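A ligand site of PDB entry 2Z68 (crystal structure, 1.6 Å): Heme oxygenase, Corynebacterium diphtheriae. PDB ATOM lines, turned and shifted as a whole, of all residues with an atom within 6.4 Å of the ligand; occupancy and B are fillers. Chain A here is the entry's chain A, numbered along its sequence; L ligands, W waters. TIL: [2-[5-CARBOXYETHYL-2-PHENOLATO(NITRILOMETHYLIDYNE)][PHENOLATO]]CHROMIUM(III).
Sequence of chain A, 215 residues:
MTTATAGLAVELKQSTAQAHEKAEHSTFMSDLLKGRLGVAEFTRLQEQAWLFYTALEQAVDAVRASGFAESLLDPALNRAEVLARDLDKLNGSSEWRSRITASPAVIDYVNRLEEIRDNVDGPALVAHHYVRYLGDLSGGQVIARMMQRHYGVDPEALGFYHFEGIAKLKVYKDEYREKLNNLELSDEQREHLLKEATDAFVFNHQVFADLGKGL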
ATOM      1  N   ALA A   9      13.830 -11.011   5.757  1.00  0.00           N
ATOM      2  CA  ALA A   9      14.938 -10.184   5.254  1.00  0.00           C
ATOM      3  C   ALA A   9      16.251 -10.949   5.442  1.00  0.00           C
ATOM      4  O   ALA A   9      17.087 -11.021   4.532  1.00  0.00           O
ATOM      5  CB  ALA A   9      14.974  -8.806   5.962  1.00  0.00           C
ATOM      6  N   VAL A  10      16.391 -11.583   6.609  1.00  0.00           N
ATOM      7  CA  VAL A  10      17.567 -12.409   6.878  1.00  0.00           C
ATOM      8  C   VAL A  10      17.605 -13.665   6.014  1.00  0.00           C
ATOM      9  O   VAL A  10      18.658 -14.024   5.472  1.00  0.00           O
ATOM     10  CB  VAL A  10      17.659 -12.780   8.374  1.00  0.00           C
ATOM     11  CG1 VAL A  10      18.761 -13.813   8.629  1.00  0.00           C
ATOM     12  CG2 VAL A  10      17.897 -11.537   9.213  1.00  0.00           C
ATOM     13  N   LYS A  13      18.811 -12.962   2.454  1.00  0.00           N
ATOM     14  CA  LYS A  13      20.269 -12.815   2.331  1.00  0.00           C
ATOM     15  C   LYS A  13      20.967 -14.172   2.314  1.00  0.00           C
ATOM     16  O   LYS A  13      21.784 -14.440   1.452  1.00  0.00           O
ATOM     17  CB  LYS A  13      20.821 -11.931   3.424  1.00  0.00           C
ATOM     18  N   HIS A  20      24.234 -14.263  -5.481  1.00  0.00           N
ATOM     19  CA  HIS A  20      24.538 -12.856  -5.276  1.00  0.00           C
ATOM     20  C   HIS A  20      26.038 -12.585  -5.341  1.00  0.00           C
ATOM     21  O   HIS A  20      26.486 -11.657  -6.035  1.00  0.00           O
ATOM     22  CB  HIS A  20      24.012 -12.437  -3.912  1.00  0.00           C
ATOM     23  CG  HIS A  20      24.028 -10.970  -3.663  1.00  0.00           C
ATOM     24  ND1 HIS A  20      23.528 -10.422  -2.508  1.00  0.00           N
ATOM     25  CD2 HIS A  20      24.459  -9.937  -4.422  1.00  0.00           C
ATOM     26  CE1 HIS A  20      23.656  -9.107  -2.557  1.00  0.00           C
ATOM     27  NE2 HIS A  20      24.211  -8.779  -3.709  1.00  0.00           N
ATOM     28  N   ALA A  23      27.083 -12.641  -8.826  1.00  0.00           N
ATOM     29  CA  ALA A  23      26.550 -11.474  -9.527  1.00  0.00           C
ATOM     30  C   ALA A  23      27.363 -10.205  -9.295  1.00  0.00           C
ATOM     31  O   ALA A  23      27.367  -9.329 -10.150  1.00  0.00           O
ATOM     32  CB  ALA A  23      25.082 -11.234  -9.154  1.00  0.00           C
ATOM     33  N   GLU A  24      28.021 -10.106  -8.138  1.00  0.00           N
ATOM     34  CA  GLU A  24      28.843  -8.938  -7.819  1.00  0.00           C
ATOM     35  C   GLU A  24      30.277  -9.079  -8.327  1.00  0.00           C
ATOM     36  O   GLU A  24      31.095  -8.182  -8.130  1.00  0.00           O
ATOM     37  CB  GLU A  24      28.858  -8.671  -6.312  1.00  0.00           C
ATOM     38  CG  GLU A  24      27.516  -8.122  -5.852  1.00  0.00           C
ATOM     39  CD  GLU A  24      27.488  -7.628  -4.408  1.00  0.00           C
ATOM     40  OE1 GLU A  24      28.494  -7.808  -3.681  1.00  0.00           O
ATOM     41  OE2 GLU A  24      26.466  -7.051  -4.005  1.00  0.00           O
ATOM     42  N   TYR A 130      13.103  -6.531  -4.295  1.00  0.00           N
ATOM     43  CA  TYR A 130      14.265  -6.631  -3.400  1.00  0.00           C
ATOM     44  C   TYR A 130      15.613  -6.527  -4.123  1.00  0.00           C
ATOM     45  O   TYR A 130      16.453  -5.667  -3.799  1.00  0.00           O
ATOM     46  CB  TYR A 130      14.162  -7.947  -2.634  1.00  0.00           C
ATOM     47  CG  TYR A 130      15.361  -8.326  -1.816  1.00  0.00           C
ATOM     48  CD1 TYR A 130      15.554  -7.804  -0.514  1.00  0.00           C
ATOM     49  CD2 TYR A 130      16.283  -9.254  -2.297  1.00  0.00           C
ATOM     50  CE1 TYR A 130      16.647  -8.188   0.242  1.00  0.00           C
ATOM     51  CE2 TYR A 130      17.378  -9.648  -1.544  1.00  0.00           C
ATOM     52  CZ  TYR A 130      17.559  -9.116  -0.289  1.00  0.00           C
ATOM     53  OH  TYR A 130      18.644  -9.516   0.442  1.00  0.00           O
ATOM     54  N   VAL A 131      15.824  -7.394  -5.105  1.00  0.00           N
ATOM     55  CA  VAL A 131      17.105  -7.456  -5.798  1.00  0.00           C
ATOM     56  C   VAL A 131      17.473  -6.114  -6.441  1.00  0.00           C
ATOM     57  O   VAL A 131      18.608  -5.644  -6.287  1.00  0.00           O
ATOM     58  CB  VAL A 131      17.157  -8.623  -6.826  1.00  0.00           C
ATOM     59  CG1 VAL A 131      18.392  -8.523  -7.712  1.00  0.00           C
ATOM     60  CG2 VAL A 131      17.097  -9.961  -6.084  1.00  0.00           C
ATOM     61  N   ARG A 132      16.504  -5.482  -7.114  1.00  0.00           N
ATOM     62  CA  ARG A 132      16.759  -4.201  -7.801  1.00  0.00           C
ATOM     63  C   ARG A 132      16.761  -3.039  -6.824  1.00  0.00           C
ATOM     64  O   ARG A 132      17.822  -2.454  -6.566  1.00  0.00           O
ATOM     65  CB  ARG A 132      15.877  -3.981  -9.042  1.00  0.00           C
ATOM     66  CG  ARG A 132      16.251  -4.849 -10.288  1.00  0.00           C
ATOM     67  CD  ARG A 132      17.746  -4.906 -10.640  1.00  0.00           C
ATOM     68  NE  ARG A 132      18.379  -3.587 -10.611  1.00  0.00           N
ATOM     69  CZ  ARG A 132      19.625  -3.335 -11.016  1.00  0.00           C
ATOM     70  NH1 ARG A 132      20.384  -4.308 -11.540  1.00  0.00           N
ATOM     71  NH2 ARG A 132      20.123  -2.105 -10.912  1.00  0.00           N
ATOM     72  N   TYR A 133      15.618  -2.730  -6.224  1.00  0.00           N
ATOM     73  CA  TYR A 133      15.498  -1.514  -5.440  1.00  0.00           C
ATOM     74  C   TYR A 133      16.266  -1.516  -4.113  1.00  0.00           C
ATOM     75  O   TYR A 133      16.841  -0.478  -3.759  1.00  0.00           O
ATOM     76  CB  TYR A 133      14.029  -1.157  -5.181  1.00  0.00           C
ATOM     77  CG  TYR A 133      13.272  -0.948  -6.467  1.00  0.00           C
ATOM     78  CD1 TYR A 133      13.561   0.137  -7.330  1.00  0.00           C
ATOM     79  CD2 TYR A 133      12.283  -1.859  -6.852  1.00  0.00           C
ATOM     80  CE1 TYR A 133      12.836   0.303  -8.548  1.00  0.00           C
ATOM     81  CE2 TYR A 133      11.583  -1.708  -8.039  1.00  0.00           C
ATOM     82  CZ  TYR A 133      11.840  -0.640  -8.881  1.00  0.00           C
ATOM     83  OH  TYR A 133      11.093  -0.555 -10.019  1.00  0.00           O
ATOM     84  N   LEU A 134      16.255  -2.617  -3.355  1.00  0.00           N
ATOM     85  CA  LEU A 134      17.027  -2.580  -2.107  1.00  0.00           C
ATOM     86  C   LEU A 134      18.526  -2.573  -2.423  1.00  0.00           C
ATOM     87  O   LEU A 134      19.318  -1.921  -1.730  1.00  0.00           O
ATOM     88  CB  LEU A 134      16.666  -3.697  -1.126  1.00  0.00           C
ATOM     89  CG  LEU A 134      17.227  -3.479   0.291  1.00  0.00           C
ATOM     90  CD1 LEU A 134      16.664  -2.189   0.898  1.00  0.00           C
ATOM     91  CD2 LEU A 134      16.894  -4.649   1.199  1.00  0.00           C
ATOM     92  N   GLY A 135      18.913  -3.273  -3.490  1.00  0.00           N
ATOM     93  CA  GLY A 135      20.258  -3.144  -4.048  1.00  0.00           C
ATOM     94  C   GLY A 135      20.632  -1.718  -4.419  1.00  0.00           C
ATOM     95  O   GLY A 135      21.727  -1.252  -4.074  1.00  0.00           O
ATOM     96  N   ASP A 136      19.739  -1.019  -5.130  1.00  0.00           N
ATOM     97  CA  ASP A 136      19.956   0.367  -5.566  1.00  0.00           C
ATOM     98  C   ASP A 136      20.067   1.279  -4.340  1.00  0.00           C
ATOM     99  O   ASP A 136      20.957   2.130  -4.284  1.00  0.00           O
ATOM    100  CB  ASP A 136      18.802   0.911  -6.420  1.00  0.00           C
ATOM    101  CG  ASP A 136      18.659   0.217  -7.756  1.00  0.00           C
ATOM    102  OD1 ASP A 136      17.542   0.298  -8.312  1.00  0.00           O
ATOM    103  OD2 ASP A 136      19.621  -0.415  -8.266  1.00  0.00           O
ATOM    104  N   SER A 138      20.983   0.487  -1.364  1.00  0.00           N
ATOM    105  CA  SER A 138      22.124   0.096  -0.556  1.00  0.00           C
ATOM    106  C   SER A 138      23.431   0.563  -1.170  1.00  0.00           C
ATOM    107  O   SER A 138      24.306   1.050  -0.441  1.00  0.00           O
ATOM    108  CB  SER A 138      22.167  -1.429  -0.424  1.00  0.00           C
ATOM    109  OG  SER A 138      21.099  -1.916   0.371  1.00  0.00           O
ATOM    110  N   ARG A 177      13.134  -3.339   5.023  1.00  0.00           N
ATOM    111  CA  ARG A 177      13.363  -4.696   5.535  1.00  0.00           C
ATOM    112  C   ARG A 177      12.264  -5.151   6.500  1.00  0.00           C
ATOM    113  O   ARG A 177      11.868  -6.323   6.499  1.00  0.00           O
ATOM    114  CB  ARG A 177      14.736  -4.811   6.201  1.00  0.00           C
ATOM    115  CG  ARG A 177      15.851  -4.908   5.184  1.00  0.00           C
ATOM    116  CD  ARG A 177      17.226  -5.149   5.817  1.00  0.00           C
ATOM    117  NE  ARG A 177      17.752  -3.922   6.411  1.00  0.00           N
ATOM    118  CZ  ARG A 177      18.578  -3.073   5.798  1.00  0.00           C
ATOM    119  NH1 ARG A 177      19.020  -3.314   4.575  1.00  0.00           N
ATOM    120  NH2 ARG A 177      18.971  -1.978   6.430  1.00  0.00           N
ATOM    121  N   LEU A 180       9.294  -6.309   4.579  1.00  0.00           N
ATOM    122  CA  LEU A 180       9.532  -7.686   4.156  1.00  0.00           C
ATOM    123  C   LEU A 180       9.218  -8.673   5.267  1.00  0.00           C
ATOM    124  O   LEU A 180       8.520  -9.656   5.040  1.00  0.00           O
ATOM    125  CB  LEU A 180      10.997  -7.877   3.794  1.00  0.00           C
ATOM    126  CG  LEU A 180      11.462  -7.198   2.508  1.00  0.00           C
ATOM    127  CD1 LEU A 180      12.983  -7.324   2.386  1.00  0.00           C
ATOM    128  CD2 LEU A 180      10.755  -7.790   1.288  1.00  0.00           C
ATOM    129  N   ALA A 200      16.613 -14.041  -9.912  1.00  0.00           N
ATOM    130  CA  ALA A 200      16.807 -12.619 -10.236  1.00  0.00           C
ATOM    131  C   ALA A 200      18.294 -12.214 -10.220  1.00  0.00           C
ATOM    132  O   ALA A 200      18.764 -11.451 -11.090  1.00  0.00           O
ATOM    133  CB  ALA A 200      15.998 -11.731  -9.296  1.00  0.00           C
ATOM    134  N   PHE A 201      19.047 -12.706  -9.234  1.00  0.00           N
ATOM    135  CA  PHE A 201      20.470 -12.426  -9.187  1.00  0.00           C
ATOM    136  C   PHE A 201      21.162 -13.019 -10.394  1.00  0.00           C
ATOM    137  O   PHE A 201      22.033 -12.379 -10.976  1.00  0.00           O
ATOM    138  CB  PHE A 201      21.076 -12.976  -7.899  1.00  0.00           C
ATOM    139  CG  PHE A 201      20.900 -12.068  -6.717  1.00  0.00           C
ATOM    140  CD1 PHE A 201      20.126 -12.464  -5.621  1.00  0.00           C
ATOM    141  CD2 PHE A 201      21.501 -10.800  -6.703  1.00  0.00           C
ATOM    142  CE1 PHE A 201      19.954 -11.601  -4.514  1.00  0.00           C
ATOM    143  CE2 PHE A 201      21.351  -9.953  -5.608  1.00  0.00           C
ATOM    144  CZ  PHE A 201      20.585 -10.349  -4.506  1.00  0.00           C
ATOM    145  N   ASN A 204      20.601 -10.958 -13.498  1.00  0.00           N
ATOM    146  CA  ASN A 204      21.463  -9.769 -13.448  1.00  0.00           C
ATOM    147  C   ASN A 204      22.920 -10.053 -13.763  1.00  0.00           C
ATOM    148  O   ASN A 204      23.580  -9.261 -14.465  1.00  0.00           O
ATOM    149  CB  ASN A 204      21.295  -9.036 -12.121  1.00  0.00           C
ATOM    150  CG  ASN A 204      20.092  -8.138 -12.125  1.00  0.00           C
ATOM    151  OD1 ASN A 204      20.154  -7.010 -12.658  1.00  0.00           O
ATOM    152  ND2 ASN A 204      18.950  -8.622 -11.605  1.00  0.00           N
ATOM    153  N   HIS A 205      23.431 -11.171 -13.253  1.00  0.00           N
ATOM    154  CA  HIS A 205      24.791 -11.618 -13.563  1.00  0.00           C
ATOM    155  C   HIS A 205      24.919 -11.757 -15.087  1.00  0.00           C
ATOM    156  O   HIS A 205      25.904 -11.278 -15.686  1.00  0.00           O
ATOM    157  CB  HIS A 205      25.040 -12.951 -12.867  1.00  0.00           C
ATOM    158  CG  HIS A 205      26.444 -13.451 -12.967  1.00  0.00           C
ATOM    159  ND1 HIS A 205      27.416 -12.859 -13.759  1.00  0.00           N
ATOM    160  CD2 HIS A 205      27.050 -14.516 -12.376  1.00  0.00           C
ATOM    161  CE1 HIS A 205      28.557 -13.532 -13.636  1.00  0.00           C
ATOM    162  NE2 HIS A 205      28.357 -14.541 -12.809  1.00  0.00           N
ATOM    163  N   PHE A 208      25.340  -8.597 -17.075  1.00  0.00           N
ATOM    164  CA  PHE A 208      26.726  -8.101 -17.038  1.00  0.00           C
ATOM    165  C   PHE A 208      27.593  -8.933 -17.979  1.00  0.00           C
ATOM    166  O   PHE A 208      28.509  -8.415 -18.599  1.00  0.00           O
ATOM    167  CB  PHE A 208      27.354  -8.211 -15.645  1.00  0.00           C
ATOM    168  CG  PHE A 208      26.701  -7.354 -14.597  1.00  0.00           C
ATOM    169  CD1 PHE A 208      26.234  -6.075 -14.889  1.00  0.00           C
ATOM    170  CD2 PHE A 208      26.644  -7.811 -13.278  1.00  0.00           C
ATOM    171  CE1 PHE A 208      25.632  -5.284 -13.897  1.00  0.00           C
ATOM    172  CE2 PHE A 208      26.038  -7.034 -12.266  1.00  0.00           C
ATOM    173  CZ  PHE A 208      25.534  -5.755 -12.576  1.00  0.00           C
HETATM  174  O2A TIL L   1      18.881  -6.918   3.208  1.00  0.00           O
HETATM  175  CGA TIL L   1      19.838  -6.272   2.727  1.00  0.00           C
HETATM  176  O1A TIL L   1      20.301  -5.267   3.325  1.00  0.00           O
HETATM  177  CBA TIL L   1      20.446  -6.684   1.407  1.00  0.00           C
HETATM  178  CAA TIL L   1      20.439  -5.468   0.493  1.00  0.00           C
HETATM  179  CC5 TIL L   1      20.957  -5.759  -0.894  1.00  0.00           C
HETATM  180  CC6 TIL L   1      22.333  -5.730  -1.120  1.00  0.00           C
HETATM  181  CC1 TIL L   1      22.807  -5.986  -2.400  1.00  0.00           C
HETATM  182  CC2 TIL L   1      21.963  -6.261  -3.430  1.00  0.00           C
HETATM  183  CC3 TIL L   1      20.568  -6.327  -3.231  1.00  0.00           C
HETATM  184  CC4 TIL L   1      20.063  -6.044  -1.942  1.00  0.00           C
HETATM  185  OA  TIL L   1      24.117  -6.016  -2.806  1.00  0.00           O
HETATM  186 CR   TIL L   1      24.501  -6.809  -4.437  1.00  0.00          CR
HETATM  187  NB  TIL L   1      22.672  -6.492  -4.599  1.00  0.00           N
HETATM  188  OB  TIL L   1      24.625  -7.382  -6.183  1.00  0.00           O
HETATM  189  CB2 TIL L   1      23.761  -7.183  -7.227  1.00  0.00           C
HETATM  190  CB1 TIL L   1      22.469  -6.716  -7.029  1.00  0.00           C
HETATM  191  CB  TIL L   1      21.989  -6.406  -5.671  1.00  0.00           C
HETATM  192  CB3 TIL L   1      24.180  -7.481  -8.525  1.00  0.00           C
HETATM  193  CB4 TIL L   1      23.328  -7.292  -9.616  1.00  0.00           C
HETATM  194  CB5 TIL L   1      22.034  -6.805  -9.413  1.00  0.00           C
HETATM  195  CB6 TIL L   1      21.600  -6.509  -8.114  1.00  0.00           C
HETATM  196  O   HOH W   1      24.799  -4.840  -5.064  1.00  0.00           O
HETATM  197  O   HOH W   2      24.910  -3.216  -1.227  1.00  0.00           O
HETATM  198  O   HOH W   3      21.383  -9.550  -0.021  1.00  0.00           O
HETATM  199  O   HOH W   4      18.354  -9.292   3.019  1.00  0.00           O
HETATM  200  O   HOH W   5      25.604  -7.306  -0.576  1.00  0.00           O
HETATM  201  O   HOH W   6      24.014  -2.604  -3.517  1.00  0.00           O
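CR of the ligand is bound by NE2 of His 20 (2.1 Å). The guanidinium group of Arg 177 lies within salt-bridge range of an oxygen (O1A) of the ligand, at 2.6 Å. A chromium atom (CR) of the ligand is bound by the side-chain carboxylate (OE2) of Glu 24.
Water W4 lies within hydrogen-bond range of an oxygen (O2A) of the ligand (2.4 Å), the side-chain hydroxyl of Tyr 130 (2.6 Å) and the backbone carbonyl oxygen of Ala 9 (2.6 Å). Water W3 bridges the side-chain hydroxyl of Tyr 130 (2.8 Å) and a ring nitrogen (ND1) of His 20 (3.4 Å).
The side-chain amide oxygen of Asn 204 is in hydrogen-bond range of the guanidinium group of Arg 132 (2.9 Å). N of Gly 135 is in hydrogen-bond range of O of Tyr 130 (3.4 Å). ND2 of Asn 204 sits at hydrogen-bond distance from O of Ala 200, 2.9 Å away. OD2 of Asp 136 is in salt-bridge range of NH2 of Arg 132, at 3.2 Å. The backbone carbonyl oxygen of Leu 134 is in hydrogen-bond range of the side-chain hydroxyl of Ser 138 (2.8 Å).
CB of Ala 23 touches CB3 of the ligand, at 3.9 Å. Tyr 130 touches the ligand. Val 131 touches the ligand. Arg 132 touches the ligand. Leu 134 touches the ligand (CD2 to O2A, 3.6 Å). Gly 135 touches the ligand. Ser 138 touches the ligand (OG to CAA, 3.6 Å). CE2 of Phe 201 touches CB of the ligand, at 3.6 Å. Asn 204 touches the ligand. CE2 of Phe 208 touches CB4 of the ligand (3.8 Å). Hydrophobic or aromatic side chains that line the ligand: His 20, Ala 23, Tyr 130, Val 131, Leu 134, Phe 201 and Phe 208. Of the 21 residues printed, 13 come within 4 Å of the ligand.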
